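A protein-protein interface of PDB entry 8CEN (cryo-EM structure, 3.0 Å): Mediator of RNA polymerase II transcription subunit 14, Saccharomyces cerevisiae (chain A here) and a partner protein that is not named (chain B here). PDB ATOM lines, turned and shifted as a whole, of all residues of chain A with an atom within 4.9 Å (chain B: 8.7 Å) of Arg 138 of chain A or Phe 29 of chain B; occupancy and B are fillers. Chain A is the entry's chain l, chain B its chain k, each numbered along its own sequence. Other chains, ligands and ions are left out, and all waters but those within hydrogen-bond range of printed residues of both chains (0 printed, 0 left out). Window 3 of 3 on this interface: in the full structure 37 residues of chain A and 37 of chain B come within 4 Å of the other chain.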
ATOM      1  N   ILE A 134      12.017  -5.382 -15.431  1.00  0.00           N
ATOM      2  CA  ILE A 134      11.926  -6.836 -15.330  1.00  0.00           C
ATOM      3  C   ILE A 134      10.563  -7.342 -15.807  1.00  0.00           C
ATOM      4  O   ILE A 134      10.470  -8.466 -16.304  1.00  0.00           O
ATOM      5  CB  ILE A 134      12.258  -7.343 -13.912  1.00  0.00           C
ATOM      6  CG1 ILE A 134      11.267  -6.830 -12.871  1.00  0.00           C
ATOM      7  CG2 ILE A 134      13.688  -6.975 -13.535  1.00  0.00           C
ATOM      8  CD1 ILE A 134      11.423  -7.478 -11.511  1.00  0.00           C
ATOM      9  N   ILE A 135       9.498  -6.535 -15.710  1.00  0.00           N
ATOM     10  CA  ILE A 135       8.234  -6.922 -16.346  1.00  0.00           C
ATOM     11  C   ILE A 135       8.363  -6.884 -17.870  1.00  0.00           C
ATOM     12  O   ILE A 135       7.793  -7.726 -18.580  1.00  0.00           O
ATOM     13  CB  ILE A 135       7.073  -6.040 -15.837  1.00  0.00           C
ATOM     14  CG1 ILE A 135       6.912  -6.167 -14.320  1.00  0.00           C
ATOM     15  CG2 ILE A 135       5.756  -6.402 -16.509  1.00  0.00           C
ATOM     16  CD1 ILE A 135       6.592  -7.555 -13.842  1.00  0.00           C
ATOM     17  N   PHE A 136       9.126  -5.921 -18.398  1.00  0.00           N
ATOM     18  CA  PHE A 136       9.403  -5.888 -19.832  1.00  0.00           C
ATOM     19  C   PHE A 136      10.150  -7.141 -20.283  1.00  0.00           C
ATOM     20  O   PHE A 136       9.801  -7.756 -21.302  1.00  0.00           O
ATOM     21  CB  PHE A 136      10.208  -4.630 -20.167  1.00  0.00           C
ATOM     22  CG  PHE A 136      10.377  -4.384 -21.638  1.00  0.00           C
ATOM     23  CD1 PHE A 136       9.374  -3.768 -22.366  1.00  0.00           C
ATOM     24  CD2 PHE A 136      11.545  -4.751 -22.288  1.00  0.00           C
ATOM     25  CE1 PHE A 136       9.528  -3.532 -23.715  1.00  0.00           C
ATOM     26  CE2 PHE A 136      11.704  -4.519 -23.641  1.00  0.00           C
ATOM     27  CZ  PHE A 136      10.693  -3.909 -24.357  1.00  0.00           C
ATOM     28  N   LEU A 137      11.164  -7.548 -19.516  1.00  0.00           N
ATOM     29  CA  LEU A 137      11.930  -8.744 -19.864  1.00  0.00           C
ATOM     30  C   LEU A 137      11.083 -10.000 -19.701  1.00  0.00           C
ATOM     31  O   LEU A 137      11.222 -10.953 -20.477  1.00  0.00           O
ATOM     32  CB  LEU A 137      13.184  -8.834 -18.999  1.00  0.00           C
ATOM     33  CG  LEU A 137      14.150  -7.659 -19.157  1.00  0.00           C
ATOM     34  CD1 LEU A 137      15.440  -7.894 -18.375  1.00  0.00           C
ATOM     35  CD2 LEU A 137      14.397  -7.296 -20.620  1.00  0.00           C
ATOM     36  N   ARG A 138      10.213 -10.007 -18.687  1.00  0.00           N
ATOM     37  CA  ARG A 138       9.205 -11.043 -18.502  1.00  0.00           C
ATOM     38  C   ARG A 138       8.380 -11.237 -19.764  1.00  0.00           C
ATOM     39  O   ARG A 138       8.223 -12.358 -20.259  1.00  0.00           O
ATOM     40  CB  ARG A 138       8.292 -10.623 -17.353  1.00  0.00           C
ATOM     41  CG  ARG A 138       7.264 -11.616 -16.907  1.00  0.00           C
ATOM     42  CD  ARG A 138       6.483 -10.992 -15.769  1.00  0.00           C
ATOM     43  NE  ARG A 138       7.310 -10.737 -14.598  1.00  0.00           N
ATOM     44  CZ  ARG A 138       7.579 -11.637 -13.667  1.00  0.00           C
ATOM     45  NH1 ARG A 138       7.132 -12.872 -13.765  1.00  0.00           N
ATOM     46  NH2 ARG A 138       8.312 -11.286 -12.613  1.00  0.00           N
ATOM     47  N   THR A 139       7.855 -10.131 -20.298  1.00  0.00           N
ATOM     48  CA  THR A 139       7.005 -10.190 -21.481  1.00  0.00           C
ATOM     49  C   THR A 139       7.783 -10.667 -22.705  1.00  0.00           C
ATOM     50  O   THR A 139       7.302 -11.524 -23.461  1.00  0.00           O
ATOM     51  CB  THR A 139       6.385  -8.813 -21.734  1.00  0.00           C
ATOM     52  OG1 THR A 139       5.523  -8.465 -20.642  1.00  0.00           O
ATOM     53  CG2 THR A 139       5.585  -8.798 -23.031  1.00  0.00           C
ATOM     54  N   GLN A 140       9.000 -10.144 -22.901  1.00  0.00           N
ATOM     55  CA  GLN A 140       9.770 -10.517 -24.089  1.00  0.00           C
ATOM     56  C   GLN A 140      10.189 -11.985 -24.048  1.00  0.00           C
ATOM     57  O   GLN A 140      10.118 -12.686 -25.066  1.00  0.00           O
ATOM     58  CB  GLN A 140      10.996  -9.615 -24.249  1.00  0.00           C
ATOM     59  CG  GLN A 140      10.713  -8.117 -24.383  1.00  0.00           C
ATOM     60  CD  GLN A 140       9.342  -7.798 -24.956  1.00  0.00           C
ATOM     61  OE1 GLN A 140       9.088  -7.985 -26.145  1.00  0.00           O
ATOM     62  NE2 GLN A 140       8.453  -7.296 -24.108  1.00  0.00           N
ATOM     63  N   PHE A 141      10.602 -12.483 -22.879  1.00  0.00           N
ATOM     64  CA  PHE A 141      10.971 -13.889 -22.787  1.00  0.00           C
ATOM     65  C   PHE A 141       9.757 -14.811 -22.778  1.00  0.00           C
ATOM     66  O   PHE A 141       9.872 -15.959 -23.217  1.00  0.00           O
ATOM     67  CB  PHE A 141      11.849 -14.123 -21.557  1.00  0.00           C
ATOM     68  CG  PHE A 141      13.292 -13.770 -21.780  1.00  0.00           C
ATOM     69  CD1 PHE A 141      14.116 -14.604 -22.517  1.00  0.00           C
ATOM     70  CD2 PHE A 141      13.818 -12.594 -21.272  1.00  0.00           C
ATOM     71  CE1 PHE A 141      15.441 -14.278 -22.733  1.00  0.00           C
ATOM     72  CE2 PHE A 141      15.141 -12.262 -21.483  1.00  0.00           C
ATOM     73  CZ  PHE A 141      15.952 -13.103 -22.216  1.00  0.00           C
ATOM     74  N   LEU A 142       8.590 -14.327 -22.342  1.00  0.00           N
ATOM     75  CA  LEU A 142       7.362 -15.096 -22.513  1.00  0.00           C
ATOM     76  C   LEU A 142       7.012 -15.243 -23.989  1.00  0.00           C
ATOM     77  O   LEU A 142       6.564 -16.309 -24.428  1.00  0.00           O
ATOM     78  CB  LEU A 142       6.223 -14.426 -21.735  1.00  0.00           C
ATOM     79  CG  LEU A 142       4.841 -15.070 -21.570  1.00  0.00           C
ATOM     80  CD1 LEU A 142       4.218 -14.559 -20.298  1.00  0.00           C
ATOM     81  CD2 LEU A 142       3.905 -14.744 -22.729  1.00  0.00           C
ATOM     82  N   VAL B  22      14.082 -21.511 -20.699  1.00  0.00           N
ATOM     83  CA  VAL B  22      13.290 -20.284 -20.713  1.00  0.00           C
ATOM     84  C   VAL B  22      12.293 -20.278 -19.557  1.00  0.00           C
ATOM     85  O   VAL B  22      12.061 -19.238 -18.924  1.00  0.00           O
ATOM     86  CB  VAL B  22      12.607 -20.117 -22.085  1.00  0.00           C
ATOM     87  CG1 VAL B  22      11.570 -19.014 -22.057  1.00  0.00           C
ATOM     88  CG2 VAL B  22      13.648 -19.821 -23.155  1.00  0.00           C
ATOM     89  N   ALA B  23      11.721 -21.444 -19.230  1.00  0.00           N
ATOM     90  CA  ALA B  23      10.829 -21.536 -18.076  1.00  0.00           C
ATOM     91  C   ALA B  23      11.572 -21.269 -16.771  1.00  0.00           C
ATOM     92  O   ALA B  23      11.025 -20.641 -15.856  1.00  0.00           O
ATOM     93  CB  ALA B  23      10.158 -22.907 -18.040  1.00  0.00           C
ATOM     94  N   SER B  24      12.818 -21.743 -16.662  1.00  0.00           N
ATOM     95  CA  SER B  24      13.622 -21.443 -15.480  1.00  0.00           C
ATOM     96  C   SER B  24      13.924 -19.951 -15.383  1.00  0.00           C
ATOM     97  O   SER B  24      13.953 -19.383 -14.282  1.00  0.00           O
ATOM     98  CB  SER B  24      14.919 -22.251 -15.508  1.00  0.00           C
ATOM     99  OG  SER B  24      15.718 -21.891 -16.621  1.00  0.00           O
ATOM    100  N   ILE B  25      14.154 -19.304 -16.529  1.00  0.00           N
ATOM    101  CA  ILE B  25      14.377 -17.859 -16.548  1.00  0.00           C
ATOM    102  C   ILE B  25      13.129 -17.117 -16.075  1.00  0.00           C
ATOM    103  O   ILE B  25      13.211 -16.166 -15.288  1.00  0.00           O
ATOM    104  CB  ILE B  25      14.817 -17.416 -17.957  1.00  0.00           C
ATOM    105  CG1 ILE B  25      16.276 -17.798 -18.192  1.00  0.00           C
ATOM    106  CG2 ILE B  25      14.643 -15.914 -18.151  1.00  0.00           C
ATOM    107  CD1 ILE B  25      16.764 -17.455 -19.565  1.00  0.00           C
ATOM    108  N   ILE B  26      11.952 -17.559 -16.527  1.00  0.00           N
ATOM    109  CA  ILE B  26      10.697 -16.936 -16.104  1.00  0.00           C
ATOM    110  C   ILE B  26      10.440 -17.176 -14.613  1.00  0.00           C
ATOM    111  O   ILE B  26       9.892 -16.313 -13.920  1.00  0.00           O
ATOM    112  CB  ILE B  26       9.539 -17.438 -16.988  1.00  0.00           C
ATOM    113  CG1 ILE B  26       9.778 -17.017 -18.438  1.00  0.00           C
ATOM    114  CG2 ILE B  26       8.194 -16.883 -16.530  1.00  0.00           C
ATOM    115  CD1 ILE B  26       8.765 -17.558 -19.410  1.00  0.00           C
ATOM    116  N   GLU B  27      10.829 -18.345 -14.096  1.00  0.00           N
ATOM    117  CA  GLU B  27      10.693 -18.605 -12.662  1.00  0.00           C
ATOM    118  C   GLU B  27      11.620 -17.704 -11.843  1.00  0.00           C
ATOM    119  O   GLU B  27      11.241 -17.193 -10.776  1.00  0.00           O
ATOM    120  CB  GLU B  27      10.977 -20.082 -12.376  1.00  0.00           C
ATOM    121  CG  GLU B  27       9.821 -21.059 -12.678  1.00  0.00           C
ATOM    122  CD  GLU B  27       8.474 -20.720 -12.033  1.00  0.00           C
ATOM    123  OE1 GLU B  27       8.420 -20.005 -11.010  1.00  0.00           O
ATOM    124  OE2 GLU B  27       7.444 -21.156 -12.587  1.00  0.00           O
ATOM    125  N   SER B  28      12.844 -17.495 -12.331  1.00  0.00           N
ATOM    126  CA  SER B  28      13.724 -16.524 -11.690  1.00  0.00           C
ATOM    127  C   SER B  28      13.115 -15.129 -11.752  1.00  0.00           C
ATOM    128  O   SER B  28      13.230 -14.345 -10.798  1.00  0.00           O
ATOM    129  CB  SER B  28      15.102 -16.546 -12.346  1.00  0.00           C
ATOM    130  OG  SER B  28      15.953 -15.572 -11.771  1.00  0.00           O
ATOM    131  N   PHE B  29      12.435 -14.820 -12.858  1.00  0.00           N
ATOM    132  CA  PHE B  29      11.739 -13.545 -12.978  1.00  0.00           C
ATOM    133  C   PHE B  29      10.609 -13.409 -11.964  1.00  0.00           C
ATOM    134  O   PHE B  29      10.451 -12.339 -11.369  1.00  0.00           O
ATOM    135  CB  PHE B  29      11.233 -13.338 -14.404  1.00  0.00           C
ATOM    136  CG  PHE B  29      12.295 -12.864 -15.353  1.00  0.00           C
ATOM    137  CD1 PHE B  29      13.465 -12.295 -14.873  1.00  0.00           C
ATOM    138  CD2 PHE B  29      12.113 -12.951 -16.721  1.00  0.00           C
ATOM    139  CE1 PHE B  29      14.445 -11.844 -15.738  1.00  0.00           C
ATOM    140  CE2 PHE B  29      13.091 -12.503 -17.597  1.00  0.00           C
ATOM    141  CZ  PHE B  29      14.258 -11.948 -17.102  1.00  0.00           C
ATOM    142  N   VAL B  30       9.826 -14.474 -11.737  1.00  0.00           N
ATOM    143  CA  VAL B  30       8.710 -14.331 -10.797  1.00  0.00           C
ATOM    144  C   VAL B  30       9.256 -14.149  -9.385  1.00  0.00           C
ATOM    145  O   VAL B  30       8.685 -13.396  -8.582  1.00  0.00           O
ATOM    146  CB  VAL B  30       7.686 -15.498 -10.834  1.00  0.00           C
ATOM    147  CG1 VAL B  30       7.012 -15.656 -12.185  1.00  0.00           C
ATOM    148  CG2 VAL B  30       8.211 -16.825 -10.293  1.00  0.00           C
ATOM    149  N   GLU B  31      10.392 -14.784  -9.067  1.00  0.00           N
ATOM    150  CA  GLU B  31      10.911 -14.634  -7.711  1.00  0.00           C
ATOM    151  C   GLU B  31      11.572 -13.269  -7.489  1.00  0.00           C
ATOM    152  O   GLU B  31      11.423 -12.681  -6.411  1.00  0.00           O
ATOM    153  CB  GLU B  31      11.825 -15.801  -7.328  1.00  0.00           C
ATOM    154  CG  GLU B  31      13.106 -15.973  -8.070  1.00  0.00           C
ATOM    155  CD  GLU B  31      13.853 -17.207  -7.607  1.00  0.00           C
ATOM    156  OE1 GLU B  31      13.333 -17.919  -6.719  1.00  0.00           O
ATOM    157  OE2 GLU B  31      14.956 -17.470  -8.129  1.00  0.00           O
ATOM    158  N   LEU B  32      12.287 -12.711  -8.487  1.00  0.00           N
ATOM    159  CA  LEU B  32      12.735 -11.350  -8.175  1.00  0.00           C
ATOM    160  C   LEU B  32      11.607 -10.334  -8.304  1.00  0.00           C
ATOM    161  O   LEU B  32      11.696  -9.262  -7.697  1.00  0.00           O
ATOM    162  CB  LEU B  32      13.921 -10.818  -9.003  1.00  0.00           C
ATOM    163  CG  LEU B  32      14.063 -10.324 -10.447  1.00  0.00           C
ATOM    164  CD1 LEU B  32      15.372  -9.559 -10.522  1.00  0.00           C
ATOM    165  CD2 LEU B  32      14.133 -11.392 -11.452  1.00  0.00           C
ATOM    166  N   GLY B  33      10.535 -10.649  -9.036  1.00  0.00           N
ATOM    167  CA  GLY B  33       9.372  -9.776  -9.035  1.00  0.00           C
ATOM    168  C   GLY B  33       8.693  -9.720  -7.680  1.00  0.00           C
ATOM    169  O   GLY B  33       8.364  -8.636  -7.184  1.00  0.00           O
ATOM    170  N   VAL B  34       8.505 -10.880  -7.045  1.00  0.00           N
ATOM    171  CA  VAL B  34       7.948 -10.869  -5.696  1.00  0.00           C
ATOM    172  C   VAL B  34       8.959 -10.302  -4.698  1.00  0.00           C
ATOM    173  O   VAL B  34       8.557  -9.731  -3.678  1.00  0.00           O
ATOM    174  CB  VAL B  34       7.435 -12.276  -5.301  1.00  0.00           C
ATOM    175  CG1 VAL B  34       8.562 -13.275  -5.136  1.00  0.00           C
ATOM    176  CG2 VAL B  34       6.558 -12.221  -4.051  1.00  0.00           C
ATOM    177  N   SER B  35      10.263 -10.388  -4.994  1.00  0.00           N
ATOM    178  CA  SER B  35      11.260  -9.716  -4.160  1.00  0.00           C
ATOM    179  C   SER B  35      11.115  -8.198  -4.216  1.00  0.00           C
ATOM    180  O   SER B  35      11.211  -7.523  -3.184  1.00  0.00           O
ATOM    181  CB  SER B  35      12.667 -10.132  -4.589  1.00  0.00           C
ATOM    182  OG  SER B  35      12.835 -11.534  -4.490  1.00  0.00           O
ATOM    183  N   ILE B  36      10.902  -7.643  -5.415  1.00  0.00           N
ATOM    184  CA  ILE B  36      10.626  -6.211  -5.543  1.00  0.00           C
ATOM    185  C   ILE B  36       9.333  -5.845  -4.827  1.00  0.00           C
ATOM    186  O   ILE B  36       9.266  -4.836  -4.111  1.00  0.00           O
ATOM    187  CB  ILE B  36      10.577  -5.790  -7.026  1.00  0.00           C
ATOM    188  CG1 ILE B  36      11.904  -6.072  -7.725  1.00  0.00           C
ATOM    189  CG2 ILE B  36      10.232  -4.314  -7.160  1.00  0.00           C
ATOM    190  CD1 ILE B  36      13.054  -5.312  -7.134  1.00  0.00           C
ATOM    191  N   ASN B  52      20.130 -14.066  -7.638  1.00  0.00           N
ATOM    192  CA  ASN B  52      19.094 -14.202  -8.661  1.00  0.00           C
ATOM    193  C   ASN B  52      19.577 -13.627  -9.992  1.00  0.00           C
ATOM    194  O   ASN B  52      19.389 -14.237 -11.054  1.00  0.00           O
ATOM    195  CB  ASN B  52      17.822 -13.501  -8.171  1.00  0.00           C
ATOM    196  CG  ASN B  52      16.593 -13.775  -9.036  1.00  0.00           C
ATOM    197  OD1 ASN B  52      16.672 -14.046 -10.231  1.00  0.00           O
ATOM    198  ND2 ASN B  52      15.433 -13.701  -8.406  1.00  0.00           N
ATOM    199  N   LEU B  53      20.211 -12.454  -9.948  1.00  0.00           N
ATOM    200  CA  LEU B  53      20.825 -11.908 -11.157  1.00  0.00           C
ATOM    201  C   LEU B  53      21.947 -12.806 -11.673  1.00  0.00           C
ATOM    202  O   LEU B  53      22.104 -12.962 -12.889  1.00  0.00           O
ATOM    203  CB  LEU B  53      21.328 -10.481 -10.924  1.00  0.00           C
ATOM    204  CG  LEU B  53      20.364  -9.287 -11.047  1.00  0.00           C
ATOM    205  CD1 LEU B  53      19.874  -9.199 -12.486  1.00  0.00           C
ATOM    206  CD2 LEU B  53      19.177  -9.293 -10.097  1.00  0.00           C
ATOM    207  N   ARG B  55      22.101 -16.126 -11.454  1.00  0.00           N
ATOM    208  CA  ARG B  55      21.535 -17.287 -12.133  1.00  0.00           C
ATOM    209  C   ARG B  55      20.852 -16.894 -13.440  1.00  0.00           C
ATOM    210  O   ARG B  55      20.934 -17.648 -14.419  1.00  0.00           O
ATOM    211  CB  ARG B  55      20.594 -18.064 -11.203  1.00  0.00           C
ATOM    212  CG  ARG B  55      19.312 -17.380 -10.795  1.00  0.00           C
ATOM    213  CD  ARG B  55      18.546 -18.223  -9.794  1.00  0.00           C
ATOM    214  NE  ARG B  55      19.240 -18.302  -8.514  1.00  0.00           N
ATOM    215  CZ  ARG B  55      18.874 -19.089  -7.512  1.00  0.00           C
ATOM    216  NH1 ARG B  55      17.813 -19.875  -7.603  1.00  0.00           N
ATOM    217  NH2 ARG B  55      19.589 -19.087  -6.391  1.00  0.00           N
ATOM    218  N   ASN B  56      20.235 -15.707 -13.495  1.00  0.00           N
ATOM    219  CA  ASN B  56      19.683 -15.217 -14.759  1.00  0.00           C
ATOM    220  C   ASN B  56      20.775 -15.035 -15.809  1.00  0.00           C
ATOM    221  O   ASN B  56      20.618 -15.461 -16.965  1.00  0.00           O
ATOM    222  CB  ASN B  56      18.948 -13.896 -14.530  1.00  0.00           C
ATOM    223  CG  ASN B  56      17.571 -14.088 -13.935  1.00  0.00           C
ATOM    224  OD1 ASN B  56      16.647 -14.543 -14.608  1.00  0.00           O
ATOM    225  ND2 ASN B  56      17.427 -13.746 -12.659  1.00  0.00           N
ATOM    226  N   VAL B  57      21.902 -14.433 -15.412  1.00  0.00           N
ATOM    227  CA  VAL B  57      22.996 -14.197 -16.349  1.00  0.00           C
ATOM    228  C   VAL B  57      23.616 -15.512 -16.808  1.00  0.00           C
ATOM    229  O   VAL B  57      23.949 -15.660 -17.986  1.00  0.00           O
ATOM    230  CB  VAL B  57      24.039 -13.239 -15.738  1.00  0.00           C
ATOM    231  CG1 VAL B  57      25.237 -13.079 -16.658  1.00  0.00           C
ATOM    232  CG2 VAL B  57      23.425 -11.867 -15.546  1.00  0.00           C
ATOM    233  N   ARG B  59      22.096 -18.499 -17.002  1.00  0.00           N
ATOM    234  CA  ARG B  59      21.165 -19.164 -17.916  1.00  0.00           C
ATOM    235  C   ARG B  59      21.192 -18.517 -19.300  1.00  0.00           C
ATOM    236  O   ARG B  59      21.194 -19.223 -20.326  1.00  0.00           O
ATOM    237  CB  ARG B  59      19.750 -19.162 -17.333  1.00  0.00           C
ATOM    238  CG  ARG B  59      19.577 -20.059 -16.109  1.00  0.00           C
ATOM    239  CD  ARG B  59      18.459 -19.566 -15.198  1.00  0.00           C
ATOM    240  NE  ARG B  59      18.484 -20.221 -13.896  1.00  0.00           N
ATOM    241  CZ  ARG B  59      17.468 -20.238 -13.043  1.00  0.00           C
ATOM    242  NH1 ARG B  59      16.327 -19.631 -13.317  1.00  0.00           N
ATOM    243  NH2 ARG B  59      17.606 -20.872 -11.882  1.00  0.00           N
ATOM    244  N   LEU B  60      21.240 -17.180 -19.350  1.00  0.00           N
ATOM    245  CA  LEU B  60      21.394 -16.492 -20.632  1.00  0.00           C
ATOM    246  C   LEU B  60      22.737 -16.809 -21.280  1.00  0.00           C
ATOM    247  O   LEU B  60      22.825 -16.924 -22.508  1.00  0.00           O
ATOM    248  CB  LEU B  60      21.227 -14.984 -20.446  1.00  0.00           C
ATOM    249  CG  LEU B  60      19.833 -14.519 -20.030  1.00  0.00           C
ATOM    250  CD1 LEU B  60      19.811 -13.028 -19.738  1.00  0.00           C
ATOM    251  CD2 LEU B  60      18.857 -14.853 -21.137  1.00  0.00           C
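O of Phe 29 of chain B sits at hydrogen-bond distance from NH2 of Arg 138 of chain A, 2.7 Å away.
Ile 134 of chain A touches Gly 33 of chain B. O of Leu 137 of chain A touches CE2 of Phe 29 of chain B (3.8 Å). Arg 138 of chain A touches Val 30 of chain B (NH1 to CG1, 3.2 Å). Phe 141 of chain A touches Val 22 of chain B (O to CG1, 3.7 Å). Phe 141 of chain A touches Phe 29 of chain B (CD2 to CE2, 3.7 Å). CD2 of Leu 60 of chain B touches CZ of Phe 141 of chain A, 3.6 Å away.
Of chain B, only Phe 29 and Val 30 come within 4 Å of Arg 138 of chain A. Phe 29 of chain B touches three residues of chain A. Of the printed residues of chain A, Val 30 of chain B touches Arg 138 (3.2 Å). Of the printed residues of chain B, Leu 137 of chain A touches Phe 29 (3.8 Å). Of the printed residues of chain A, Val 22 of chain B touches Phe 141 (3.7 Å). Of the printed residues of chain B, Ile 134 of chain A touches Gly 33 (3.95 Å).
Hydrophobic or aromatic side chains of chain A that line the printed part of chain B: Ile 134, Leu 137 and Phe 141. Of the 22 printed residues of chain B, 5 touch a printed residue of chain A. Printed residues of chain B that touch a printed residue of chain A: Val 22, Phe 29, Val 30, Gly 33 and Leu 60. Hydrophobic or aromatic side chains of chain B within 4 Å of the printed part of chain A: Val 22, Phe 29, Val 30 and Leu 60. Among the printed residues, 7 pairs touch across the chains.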
